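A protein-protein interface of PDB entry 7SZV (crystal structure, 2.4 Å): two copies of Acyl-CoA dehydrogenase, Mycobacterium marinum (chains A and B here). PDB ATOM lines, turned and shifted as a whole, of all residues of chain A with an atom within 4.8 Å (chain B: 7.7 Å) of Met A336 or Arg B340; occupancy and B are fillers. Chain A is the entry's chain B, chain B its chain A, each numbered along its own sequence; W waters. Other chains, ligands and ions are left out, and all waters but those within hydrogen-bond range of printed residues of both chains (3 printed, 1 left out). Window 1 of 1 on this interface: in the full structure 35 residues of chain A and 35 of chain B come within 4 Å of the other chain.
Water W3 lies within hydrogen-bond range of OD2 of Asp B337 (2.8 Å) and NH2 of Arg A340 (2.9 Å).
Water W1 lies within hydrogen-bond range of the backbone carbonyl oxygen (O) of Met A336 (2.8 Å) and the side-chain hydroxyl (OH) of Tyr B361 (3.4 Å).
Water W2 bridges OD2 of Asp A337 and NH2 of Arg B340.
Among the printed residues, pairs that only touch across the chains: Lys A365 with Thr B343 (3.1 Å), Arg A340 with Met B336 (3.5 Å), Met A336 with Arg B340 (3.8 Å), Lys A365 with Tyr B361 (3.8 Å) and Glu A333 with Arg B340 (3.9 Å).
Met A336 touches Arg B340, and with the chains exchanged Arg A340 touches Met B336.
Asp A337 touches Arg B340, and with the chains exchanged Arg A340 touches Asp B337.
8 positions are printed for both chains.
Printed residues of chain A that touch a printed residue of chain B: Glu A333, Met A336, Asp A337, Arg A340, Lys A365 and Glu A368.
Hydrophobic or aromatic side chains of chain A within 4 Å of the printed part of chain B: Met A336.
Hydrophobic or aromatic side chains of chain B that line the printed part of chain A: Met B336 and Tyr B361.
Among the printed residues, 12 pairs touch across the chains.
O of Arg B340 is in hydrogen-bond range of NZ of Lys A365, 3.0 Å away.
OD1 of Asp A337 lies within salt-bridge range of NH1 of Arg B340 (2.9 Å).
The side-chain sulfur (SD) of Met A336 sits close to the side-chain hydroxyl (OH) of Tyr B361.
The guanidinium group of Arg B340 lies within salt-bridge range of the side-chain carboxylate of Glu A368 (2.7 Å).
The side-chain amide nitrogen (NE2) of Gln B344 sits at hydrogen-bond distance from the backbone carbonyl oxygen (O) of Glu A368 (3.1 Å).
OD1 of Asp B337 lies within salt-bridge range of NH1 of Arg A340.
The side-chain amide oxygen (OE1) of Gln B344 is in hydrogen-bond range of the side-chain amino group (NZ) of Lys A365, at 2.9 Å.
The side-chain amino group (NZ) of Lys A365 lies within salt-bridge range of the side-chain carboxylate (OE1) of Glu A368 (2.8 Å).
The side-chain hydroxyl of Thr B343 is in hydrogen-bond range of the backbone carbonyl oxygen of Arg B340 (3.1 Å).
N of Lys A365 is in hydrogen-bond range of SD of Met A336 (3.5 Å).
The backbone carbonyl oxygen (O) of Ala B339 lies within hydrogen-bond range of the side-chain hydroxyl (OG1) of Thr B343 (2.9 Å).
Met A336 touches just these residues of chain B: Arg B340 and Tyr B361.
Of chain A, only Glu A333, Met A336, Asp A337, Lys A365 and Glu A368 come within 4 Å of Arg B340.
Ala A335 touches none of the printed residues of chain B.
Of the printed residues of chain B, Arg A340 touches Met B336 and Asp B337.
Of the printed residues of chain B, Lys A365 touches Arg B340, Thr B343, Gln B344 and Tyr B361.
Of the printed residues of chain A, Gln B344 touches Lys A365 and Glu A368.
Of the printed residues of chain A, Thr B343 touches Lys A365.
Of the printed residues of chain B, Glu A368 touches Arg B340 (2.7 Å) and Gln B344 (3.1 Å).
The nearest residue of chain B that does not touch Met A336 is Thr B343 (6.2 Å).
The nearest printed residue of chain A that does not touch Arg B340 is Ser A332 (5.1 Å).
The nearest printed residue of chain A that does not touch Thr B343 is Glu A368 (6.1 Å).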
ATOM      1  N   SER A 332     -17.714 -20.175  -2.192  1.00  0.00           N
ATOM      2  CA  SER A 332     -17.312 -19.305  -3.289  1.00  0.00           C
ATOM      3  C   SER A 332     -17.857 -19.824  -4.602  1.00  0.00           C
ATOM      4  O   SER A 332     -18.241 -19.036  -5.471  1.00  0.00           O
ATOM      5  CB  SER A 332     -15.785 -19.172  -3.336  1.00  0.00           C
ATOM      6  OG  SER A 332     -15.177 -20.378  -3.733  1.00  0.00           O
ATOM      7  N   GLU A 333     -17.934 -21.155  -4.751  1.00  0.00           N
ATOM      8  CA  GLU A 333     -18.470 -21.731  -5.986  1.00  0.00           C
ATOM      9  C   GLU A 333     -19.989 -21.615  -6.042  1.00  0.00           C
ATOM     10  O   GLU A 333     -20.551 -21.447  -7.134  1.00  0.00           O
ATOM     11  CB  GLU A 333     -18.029 -23.201  -6.136  1.00  0.00           C
ATOM     12  CG  GLU A 333     -16.497 -23.274  -6.345  1.00  0.00           C
ATOM     13  CD  GLU A 333     -15.860 -24.646  -6.162  1.00  0.00           C
ATOM     14  OE1 GLU A 333     -16.514 -25.616  -5.686  1.00  0.00           O
ATOM     15  OE2 GLU A 333     -14.655 -24.727  -6.503  1.00  0.00           O
ATOM     16  N   ALA A 334     -20.665 -21.638  -4.879  1.00  0.00           N
ATOM     17  CA  ALA A 334     -22.106 -21.416  -4.871  1.00  0.00           C
ATOM     18  C   ALA A 334     -22.434 -19.982  -5.266  1.00  0.00           C
ATOM     19  O   ALA A 334     -23.399 -19.753  -6.014  1.00  0.00           O
ATOM     20  CB  ALA A 334     -22.709 -21.744  -3.501  1.00  0.00           C
ATOM     21  N   ALA A 335     -21.614 -19.014  -4.826  1.00  0.00           N
ATOM     22  CA  ALA A 335     -21.826 -17.614  -5.213  1.00  0.00           C
ATOM     23  C   ALA A 335     -21.637 -17.408  -6.715  1.00  0.00           C
ATOM     24  O   ALA A 335     -22.493 -16.809  -7.387  1.00  0.00           O
ATOM     25  CB  ALA A 335     -20.880 -16.688  -4.425  1.00  0.00           C
ATOM     26  N   MET A 336     -20.507 -17.873  -7.256  1.00  0.00           N
ATOM     27  CA  MET A 336     -20.250 -17.735  -8.692  1.00  0.00           C
ATOM     28  C   MET A 336     -21.330 -18.424  -9.507  1.00  0.00           C
ATOM     29  O   MET A 336     -21.864 -17.847 -10.470  1.00  0.00           O
ATOM     30  CB  MET A 336     -18.891 -18.348  -9.041  1.00  0.00           C
ATOM     31  CG  MET A 336     -17.731 -17.530  -8.522  1.00  0.00           C
ATOM     32  SD  MET A 336     -17.706 -16.028  -9.545  1.00  0.00           S
ATOM     33  CE  MET A 336     -16.995 -16.691 -11.065  1.00  0.00           C
ATOM     34  N   ASP A 337     -21.664 -19.676  -9.146  1.00  0.00           N
ATOM     35  CA  ASP A 337     -22.660 -20.397  -9.935  1.00  0.00           C
ATOM     36  C   ASP A 337     -24.031 -19.732  -9.828  1.00  0.00           C
ATOM     37  O   ASP A 337     -24.711 -19.558 -10.843  1.00  0.00           O
ATOM     38  CB  ASP A 337     -22.734 -21.873  -9.516  1.00  0.00           C
ATOM     39  CG  ASP A 337     -21.472 -22.690  -9.921  1.00  0.00           C
ATOM     40  OD1 ASP A 337     -20.778 -22.348 -10.912  1.00  0.00           O
ATOM     41  OD2 ASP A 337     -21.184 -23.705  -9.243  1.00  0.00           O
ATOM     42  N   ASN A 338     -24.428 -19.315  -8.616  1.00  0.00           N
ATOM     43  CA  ASN A 338     -25.730 -18.685  -8.443  1.00  0.00           C
ATOM     44  C   ASN A 338     -25.768 -17.310  -9.086  1.00  0.00           C
ATOM     45  O   ASN A 338     -26.831 -16.882  -9.543  1.00  0.00           O
ATOM     46  CB  ASN A 338     -26.107 -18.592  -6.961  1.00  0.00           C
ATOM     47  CG  ASN A 338     -26.630 -19.924  -6.414  1.00  0.00           C
ATOM     48  OD1 ASN A 338     -26.487 -20.958  -7.072  1.00  0.00           O
ATOM     49  ND2 ASN A 338     -27.219 -19.911  -5.202  1.00  0.00           N
ATOM     50  N   ALA A 339     -24.628 -16.612  -9.158  1.00  0.00           N
ATOM     51  CA  ALA A 339     -24.639 -15.321  -9.836  1.00  0.00           C
ATOM     52  C   ALA A 339     -24.804 -15.486 -11.344  1.00  0.00           C
ATOM     53  O   ALA A 339     -25.522 -14.712 -11.989  1.00  0.00           O
ATOM     54  CB  ALA A 339     -23.373 -14.540  -9.515  1.00  0.00           C
ATOM     55  N   ARG A 340     -24.139 -16.477 -11.930  1.00  0.00           N
ATOM     56  CA  ARG A 340     -24.302 -16.716 -13.359  1.00  0.00           C
ATOM     57  C   ARG A 340     -25.718 -17.185 -13.668  1.00  0.00           C
ATOM     58  O   ARG A 340     -26.297 -16.806 -14.690  1.00  0.00           O
ATOM     59  CB  ARG A 340     -23.254 -17.716 -13.819  1.00  0.00           C
ATOM     60  CG  ARG A 340     -23.367 -18.133 -15.235  1.00  0.00           C
ATOM     61  CD  ARG A 340     -22.291 -19.156 -15.593  1.00  0.00           C
ATOM     62  NE  ARG A 340     -22.413 -19.552 -16.994  1.00  0.00           N
ATOM     63  CZ  ARG A 340     -21.650 -20.454 -17.592  1.00  0.00           C
ATOM     64  NH1 ARG A 340     -20.667 -21.062 -16.944  1.00  0.00           N
ATOM     65  NH2 ARG A 340     -21.917 -20.792 -18.857  1.00  0.00           N
ATOM     66  N   SER A 364     -18.349 -11.557  -7.495  1.00  0.00           N
ATOM     67  CA  SER A 364     -18.064 -12.865  -6.925  1.00  0.00           C
ATOM     68  C   SER A 364     -16.773 -13.493  -7.435  1.00  0.00           C
ATOM     69  O   SER A 364     -16.295 -14.449  -6.816  1.00  0.00           O
ATOM     70  CB  SER A 364     -19.231 -13.808  -7.192  1.00  0.00           C
ATOM     71  OG  SER A 364     -20.379 -13.363  -6.486  1.00  0.00           O
ATOM     72  N   LYS A 365     -16.190 -13.006  -8.533  1.00  0.00           N
ATOM     73  CA  LYS A 365     -14.994 -13.679  -9.038  1.00  0.00           C
ATOM     74  C   LYS A 365     -13.882 -13.711  -7.987  1.00  0.00           C
ATOM     75  O   LYS A 365     -13.129 -14.695  -7.898  1.00  0.00           O
ATOM     76  CB  LYS A 365     -14.471 -12.992 -10.296  1.00  0.00           C
ATOM     77  CG  LYS A 365     -13.250 -13.702 -10.888  1.00  0.00           C
ATOM     78  CD  LYS A 365     -13.516 -15.195 -11.102  1.00  0.00           C
ATOM     79  CE  LYS A 365     -12.248 -16.022 -10.882  1.00  0.00           C
ATOM     80  NZ  LYS A 365     -12.412 -17.500 -11.163  1.00  0.00           N
ATOM     81  N   GLU A 368     -13.337 -16.681  -5.309  1.00  0.00           N
ATOM     82  CA  GLU A 368     -12.584 -17.898  -5.630  1.00  0.00           C
ATOM     83  C   GLU A 368     -11.090 -17.687  -5.541  1.00  0.00           C
ATOM     84  O   GLU A 368     -10.320 -18.644  -5.728  1.00  0.00           O
ATOM     85  CB  GLU A 368     -12.866 -18.365  -7.063  1.00  0.00           C
ATOM     86  CG  GLU A 368     -14.279 -18.741  -7.322  1.00  0.00           C
ATOM     87  CD  GLU A 368     -14.439 -19.445  -8.657  1.00  0.00           C
ATOM     88  OE1 GLU A 368     -14.460 -18.784  -9.726  1.00  0.00           O
ATOM     89  OE2 GLU A 368     -14.510 -20.681  -8.623  1.00  0.00           O
ATOM     90  N   CYS B 265      -9.010 -15.823 -24.007  1.00  0.00           N
ATOM     91  CA  CYS B 265      -8.776 -16.220 -22.623  1.00  0.00           C
ATOM     92  C   CYS B 265      -7.673 -17.268 -22.521  1.00  0.00           C
ATOM     93  O   CYS B 265      -6.829 -17.216 -21.613  1.00  0.00           O
ATOM     94  CB  CYS B 265     -10.082 -16.743 -22.037  1.00  0.00           C
ATOM     95  SG  CYS B 265     -11.298 -15.421 -21.821  1.00  0.00           S
ATOM     96  N   LYS B 292      -6.008 -26.960 -16.533  1.00  0.00           N
ATOM     97  CA  LYS B 292      -7.112 -26.022 -16.682  1.00  0.00           C
ATOM     98  C   LYS B 292      -6.987 -25.245 -17.996  1.00  0.00           C
ATOM     99  O   LYS B 292      -7.965 -25.087 -18.740  1.00  0.00           O
ATOM    100  CB  LYS B 292      -7.109 -25.102 -15.461  1.00  0.00           C
ATOM    101  CG  LYS B 292      -8.024 -23.900 -15.475  1.00  0.00           C
ATOM    102  CD  LYS B 292      -7.672 -23.084 -14.246  1.00  0.00           C
ATOM    103  CE  LYS B 292      -8.766 -23.149 -13.227  1.00  0.00           C
ATOM    104  NZ  LYS B 292      -9.087 -24.543 -12.832  1.00  0.00           N
ATOM    105  N   MET B 296      -9.318 -25.370 -21.348  1.00  0.00           N
ATOM    106  CA  MET B 296      -9.804 -24.140 -21.970  1.00  0.00           C
ATOM    107  C   MET B 296      -9.578 -24.197 -23.473  1.00  0.00           C
ATOM    108  O   MET B 296     -10.448 -23.799 -24.267  1.00  0.00           O
ATOM    109  CB  MET B 296      -9.107 -22.899 -21.385  1.00  0.00           C
ATOM    110  CG  MET B 296      -9.383 -22.568 -19.892  1.00  0.00           C
ATOM    111  SD  MET B 296      -8.202 -21.349 -19.198  1.00  0.00           S
ATOM    112  CE  MET B 296      -8.569 -19.902 -20.217  1.00  0.00           C
ATOM    113  N   ARG B 299     -12.094 -26.404 -25.162  1.00  0.00           N
ATOM    114  CA  ARG B 299     -13.404 -25.762 -25.321  1.00  0.00           C
ATOM    115  C   ARG B 299     -13.425 -24.818 -26.517  1.00  0.00           C
ATOM    116  O   ARG B 299     -14.386 -24.794 -27.286  1.00  0.00           O
ATOM    117  CB  ARG B 299     -13.787 -24.984 -24.063  1.00  0.00           C
ATOM    118  CG  ARG B 299     -14.037 -25.814 -22.827  1.00  0.00           C
ATOM    119  CD  ARG B 299     -14.370 -24.854 -21.658  1.00  0.00           C
ATOM    120  NE  ARG B 299     -14.328 -25.480 -20.336  1.00  0.00           N
ATOM    121  CZ  ARG B 299     -13.776 -24.931 -19.259  1.00  0.00           C
ATOM    122  NH1 ARG B 299     -13.139 -23.766 -19.320  1.00  0.00           N
ATOM    123  NH2 ARG B 299     -13.877 -25.558 -18.090  1.00  0.00           N
ATOM    124  N   ALA B 334     -18.415 -21.617 -23.841  1.00  0.00           N
ATOM    125  CA  ALA B 334     -16.959 -21.674 -23.853  1.00  0.00           C
ATOM    126  C   ALA B 334     -16.375 -20.325 -23.458  1.00  0.00           C
ATOM    127  O   ALA B 334     -15.375 -20.257 -22.722  1.00  0.00           O
ATOM    128  CB  ALA B 334     -16.438 -22.111 -25.221  1.00  0.00           C
ATOM    129  N   ALA B 335     -17.007 -19.232 -23.885  1.00  0.00           N
ATOM    130  CA  ALA B 335     -16.512 -17.931 -23.446  1.00  0.00           C
ATOM    131  C   ALA B 335     -16.655 -17.781 -21.930  1.00  0.00           C
ATOM    132  O   ALA B 335     -15.676 -17.472 -21.237  1.00  0.00           O
ATOM    133  CB  ALA B 335     -17.228 -16.799 -24.193  1.00  0.00           C
ATOM    134  N   MET B 336     -17.858 -18.045 -21.390  1.00  0.00           N
ATOM    135  CA  MET B 336     -18.078 -17.892 -19.944  1.00  0.00           C
ATOM    136  C   MET B 336     -17.141 -18.782 -19.131  1.00  0.00           C
ATOM    137  O   MET B 336     -16.452 -18.311 -18.207  1.00  0.00           O
ATOM    138  CB  MET B 336     -19.544 -18.180 -19.609  1.00  0.00           C
ATOM    139  CG  MET B 336     -20.505 -17.053 -20.032  1.00  0.00           C
ATOM    140  SD  MET B 336     -20.253 -15.661 -18.892  1.00  0.00           S
ATOM    141  CE  MET B 336     -21.075 -16.361 -17.430  1.00  0.00           C
ATOM    142  N   ASP B 337     -17.045 -20.064 -19.499  1.00  0.00           N
ATOM    143  CA  ASP B 337     -16.167 -20.954 -18.755  1.00  0.00           C
ATOM    144  C   ASP B 337     -14.698 -20.510 -18.880  1.00  0.00           C
ATOM    145  O   ASP B 337     -13.989 -20.420 -17.874  1.00  0.00           O
ATOM    146  CB  ASP B 337     -16.364 -22.397 -19.239  1.00  0.00           C
ATOM    147  CG  ASP B 337     -17.775 -22.959 -18.930  1.00  0.00           C
ATOM    148  OD1 ASP B 337     -18.434 -22.546 -17.949  1.00  0.00           O
ATOM    149  OD2 ASP B 337     -18.263 -23.779 -19.750  1.00  0.00           O
ATOM    150  N   ASN B 338     -14.244 -20.135 -20.087  1.00  0.00           N
ATOM    151  CA  ASN B 338     -12.832 -19.766 -20.235  1.00  0.00           C
ATOM    152  C   ASN B 338     -12.505 -18.452 -19.537  1.00  0.00           C
ATOM    153  O   ASN B 338     -11.374 -18.278 -19.052  1.00  0.00           O
ATOM    154  CB  ASN B 338     -12.434 -19.689 -21.713  1.00  0.00           C
ATOM    155  CG  ASN B 338     -12.186 -21.074 -22.322  1.00  0.00           C
ATOM    156  OD1 ASN B 338     -12.558 -22.096 -21.734  1.00  0.00           O
ATOM    157  ND2 ASN B 338     -11.516 -21.115 -23.478  1.00  0.00           N
ATOM    158  N   ALA B 339     -13.477 -17.536 -19.438  1.00  0.00           N
ATOM    159  CA  ALA B 339     -13.246 -16.299 -18.699  1.00  0.00           C
ATOM    160  C   ALA B 339     -13.127 -16.560 -17.199  1.00  0.00           C
ATOM    161  O   ALA B 339     -12.350 -15.900 -16.498  1.00  0.00           O
ATOM    162  CB  ALA B 339     -14.372 -15.304 -18.988  1.00  0.00           C
ATOM    163  N   ARG B 340     -13.946 -17.450 -16.669  1.00  0.00           N
ATOM    164  CA  ARG B 340     -13.811 -17.776 -15.265  1.00  0.00           C
ATOM    165  C   ARG B 340     -12.504 -18.508 -15.002  1.00  0.00           C
ATOM    166  O   ARG B 340     -11.868 -18.281 -13.973  1.00  0.00           O
ATOM    167  CB  ARG B 340     -15.032 -18.567 -14.811  1.00  0.00           C
ATOM    168  CG  ARG B 340     -14.961 -19.056 -13.391  1.00  0.00           C
ATOM    169  CD  ARG B 340     -16.274 -19.837 -13.029  1.00  0.00           C
ATOM    170  NE  ARG B 340     -16.157 -20.321 -11.661  1.00  0.00           N
ATOM    171  CZ  ARG B 340     -17.061 -21.063 -11.050  1.00  0.00           C
ATOM    172  NH1 ARG B 340     -18.183 -21.417 -11.663  1.00  0.00           N
ATOM    173  NH2 ARG B 340     -16.836 -21.456  -9.788  1.00  0.00           N
ATOM    174  N   ASP B 341     -12.047 -19.323 -15.940  1.00  0.00           N
ATOM    175  CA  ASP B 341     -10.776 -20.012 -15.712  1.00  0.00           C
ATOM    176  C   ASP B 341      -9.592 -19.075 -15.909  1.00  0.00           C
ATOM    177  O   ASP B 341      -8.646 -19.098 -15.108  1.00  0.00           O
ATOM    178  CB  ASP B 341     -10.651 -21.190 -16.666  1.00  0.00           C
ATOM    179  CG  ASP B 341     -11.495 -22.389 -16.232  1.00  0.00           C
ATOM    180  OD1 ASP B 341     -11.869 -22.457 -15.036  1.00  0.00           O
ATOM    181  OD2 ASP B 341     -11.767 -23.259 -17.092  1.00  0.00           O
ATOM    182  N   ALA B 342      -9.661 -18.209 -16.938  1.00  0.00           N
ATOM    183  CA  ALA B 342      -8.561 -17.295 -17.226  1.00  0.00           C
ATOM    184  C   ALA B 342      -8.369 -16.295 -16.096  1.00  0.00           C
ATOM    185  O   ALA B 342      -7.228 -15.960 -15.751  1.00  0.00           O
ATOM    186  CB  ALA B 342      -8.788 -16.559 -18.558  1.00  0.00           C
ATOM    187  N   THR B 343      -9.466 -15.789 -15.516  1.00  0.00           N
ATOM    188  CA  THR B 343      -9.282 -14.902 -14.374  1.00  0.00           C
ATOM    189  C   THR B 343      -8.716 -15.667 -13.191  1.00  0.00           C
ATOM    190  O   THR B 343      -7.914 -15.109 -12.431  1.00  0.00           O
ATOM    191  CB  THR B 343     -10.589 -14.199 -13.973  1.00  0.00           C
ATOM    192  OG1 THR B 343     -11.622 -15.171 -13.751  1.00  0.00           O
ATOM    193  CG2 THR B 343     -11.041 -13.179 -15.074  1.00  0.00           C
ATOM    194  N   GLN B 344      -9.075 -16.949 -13.043  1.00  0.00           N
ATOM    195  CA  GLN B 344      -8.479 -17.755 -11.980  1.00  0.00           C
ATOM    196  C   GLN B 344      -6.974 -17.882 -12.192  1.00  0.00           C
ATOM    197  O   GLN B 344      -6.186 -17.632 -11.277  1.00  0.00           O
ATOM    198  CB  GLN B 344      -9.144 -19.143 -11.913  1.00  0.00           C
ATOM    199  CG  GLN B 344      -8.799 -19.960 -10.637  1.00  0.00           C
ATOM    200  CD  GLN B 344      -9.414 -19.359  -9.383  1.00  0.00           C
ATOM    201  OE1 GLN B 344     -10.305 -18.503  -9.457  1.00  0.00           O
ATOM    202  NE2 GLN B 344      -8.953 -19.794  -8.237  1.00  0.00           N
ATOM    203  N   VAL B 345      -6.558 -18.177 -13.428  1.00  0.00           N
ATOM    204  CA  VAL B 345      -5.138 -18.315 -13.729  1.00  0.00           C
ATOM    205  C   VAL B 345      -4.400 -17.024 -13.406  1.00  0.00           C
ATOM    206  O   VAL B 345      -3.288 -17.045 -12.865  1.00  0.00           O
ATOM    207  CB  VAL B 345      -4.949 -18.725 -15.201  1.00  0.00           C
ATOM    208  CG1 VAL B 345      -3.465 -18.703 -15.597  1.00  0.00           C
ATOM    209  CG2 VAL B 345      -5.593 -20.115 -15.468  1.00  0.00           C
ATOM    210  N   HIS B 346      -5.028 -15.880 -13.675  1.00  0.00           N
ATOM    211  CA  HIS B 346      -4.380 -14.603 -13.407  1.00  0.00           C
ATOM    212  C   HIS B 346      -4.435 -14.204 -11.941  1.00  0.00           C
ATOM    213  O   HIS B 346      -3.787 -13.219 -11.567  1.00  0.00           O
ATOM    214  CB  HIS B 346      -5.016 -13.494 -14.243  1.00  0.00           C
ATOM    215  CG  HIS B 346      -4.665 -13.558 -15.695  1.00  0.00           C
ATOM    216  ND1 HIS B 346      -5.066 -14.595 -16.509  1.00  0.00           N
ATOM    217  CD2 HIS B 346      -3.952 -12.713 -16.481  1.00  0.00           C
ATOM    218  CE1 HIS B 346      -4.635 -14.379 -17.742  1.00  0.00           C
ATOM    219  NE2 HIS B 346      -3.956 -13.246 -17.753  1.00  0.00           N
ATOM    220  N   VAL B 357      -8.516 -10.553 -19.686  1.00  0.00           N
ATOM    221  CA  VAL B 357      -9.409 -11.637 -19.266  1.00  0.00           C
ATOM    222  C   VAL B 357     -10.421 -11.141 -18.245  1.00  0.00           C
ATOM    223  O   VAL B 357     -11.536 -11.671 -18.168  1.00  0.00           O
ATOM    224  CB  VAL B 357      -8.615 -12.858 -18.756  1.00  0.00           C
ATOM    225  CG1 VAL B 357      -7.695 -13.371 -19.856  1.00  0.00           C
ATOM    226  CG2 VAL B 357      -7.822 -12.553 -17.452  1.00  0.00           C
ATOM    227  N   HIS B 360     -13.059  -9.781 -20.227  1.00  0.00           N
ATOM    228  CA  HIS B 360     -13.814 -10.876 -20.831  1.00  0.00           C
ATOM    229  C   HIS B 360     -14.772 -11.516 -19.816  1.00  0.00           C
ATOM    230  O   HIS B 360     -15.893 -11.907 -20.175  1.00  0.00           O
ATOM    231  CB  HIS B 360     -12.866 -11.915 -21.455  1.00  0.00           C
ATOM    232  CG  HIS B 360     -12.381 -11.544 -22.829  1.00  0.00           C
ATOM    233  ND1 HIS B 360     -13.150 -10.821 -23.724  1.00  0.00           N
ATOM    234  CD2 HIS B 360     -11.194 -11.766 -23.450  1.00  0.00           C
ATOM    235  CE1 HIS B 360     -12.466 -10.633 -24.839  1.00  0.00           C
ATOM    236  NE2 HIS B 360     -11.284 -11.211 -24.707  1.00  0.00           N
ATOM    237  N   TYR B 361     -14.377 -11.588 -18.546  1.00  0.00           N
ATOM    238  CA  TYR B 361     -15.282 -12.136 -17.540  1.00  0.00           C
ATOM    239  C   TYR B 361     -16.537 -11.278 -17.390  1.00  0.00           C
ATOM    240  O   TYR B 361     -17.634 -11.816 -17.242  1.00  0.00           O
ATOM    241  CB  TYR B 361     -14.571 -12.273 -16.196  1.00  0.00           C
ATOM    242  CG  TYR B 361     -15.522 -12.675 -15.088  1.00  0.00           C
ATOM    243  CD1 TYR B 361     -15.964 -13.994 -14.963  1.00  0.00           C
ATOM    244  CD2 TYR B 361     -15.988 -11.734 -14.167  1.00  0.00           C
ATOM    245  CE1 TYR B 361     -16.849 -14.354 -13.962  1.00  0.00           C
ATOM    246  CE2 TYR B 361     -16.866 -12.088 -13.159  1.00  0.00           C
ATOM    247  CZ  TYR B 361     -17.295 -13.406 -13.056  1.00  0.00           C
ATOM    248  OH  TYR B 361     -18.173 -13.766 -12.040  1.00  0.00           O
ATOM    249  N   SER B 364     -18.730 -11.276 -21.051  1.00  0.00           N
ATOM    250  CA  SER B 364     -19.235 -12.492 -21.668  1.00  0.00           C
ATOM    251  C   SER B 364     -20.627 -12.888 -21.191  1.00  0.00           C
ATOM    252  O   SER B 364     -21.291 -13.676 -21.890  1.00  0.00           O
ATOM    253  CB  SER B 364     -18.270 -13.640 -21.409  1.00  0.00           C
ATOM    254  OG  SER B 364     -17.042 -13.377 -22.059  1.00  0.00           O
HETATM  255  O   HOH W   1     -20.326 -16.419 -12.333  1.00  0.00           O
HETATM  256  O   HOH W   2     -18.341 -23.895  -9.437  1.00  0.00           O
HETATM  257  O   HOH W   3     -20.961 -23.446 -19.334  1.00  0.00           O
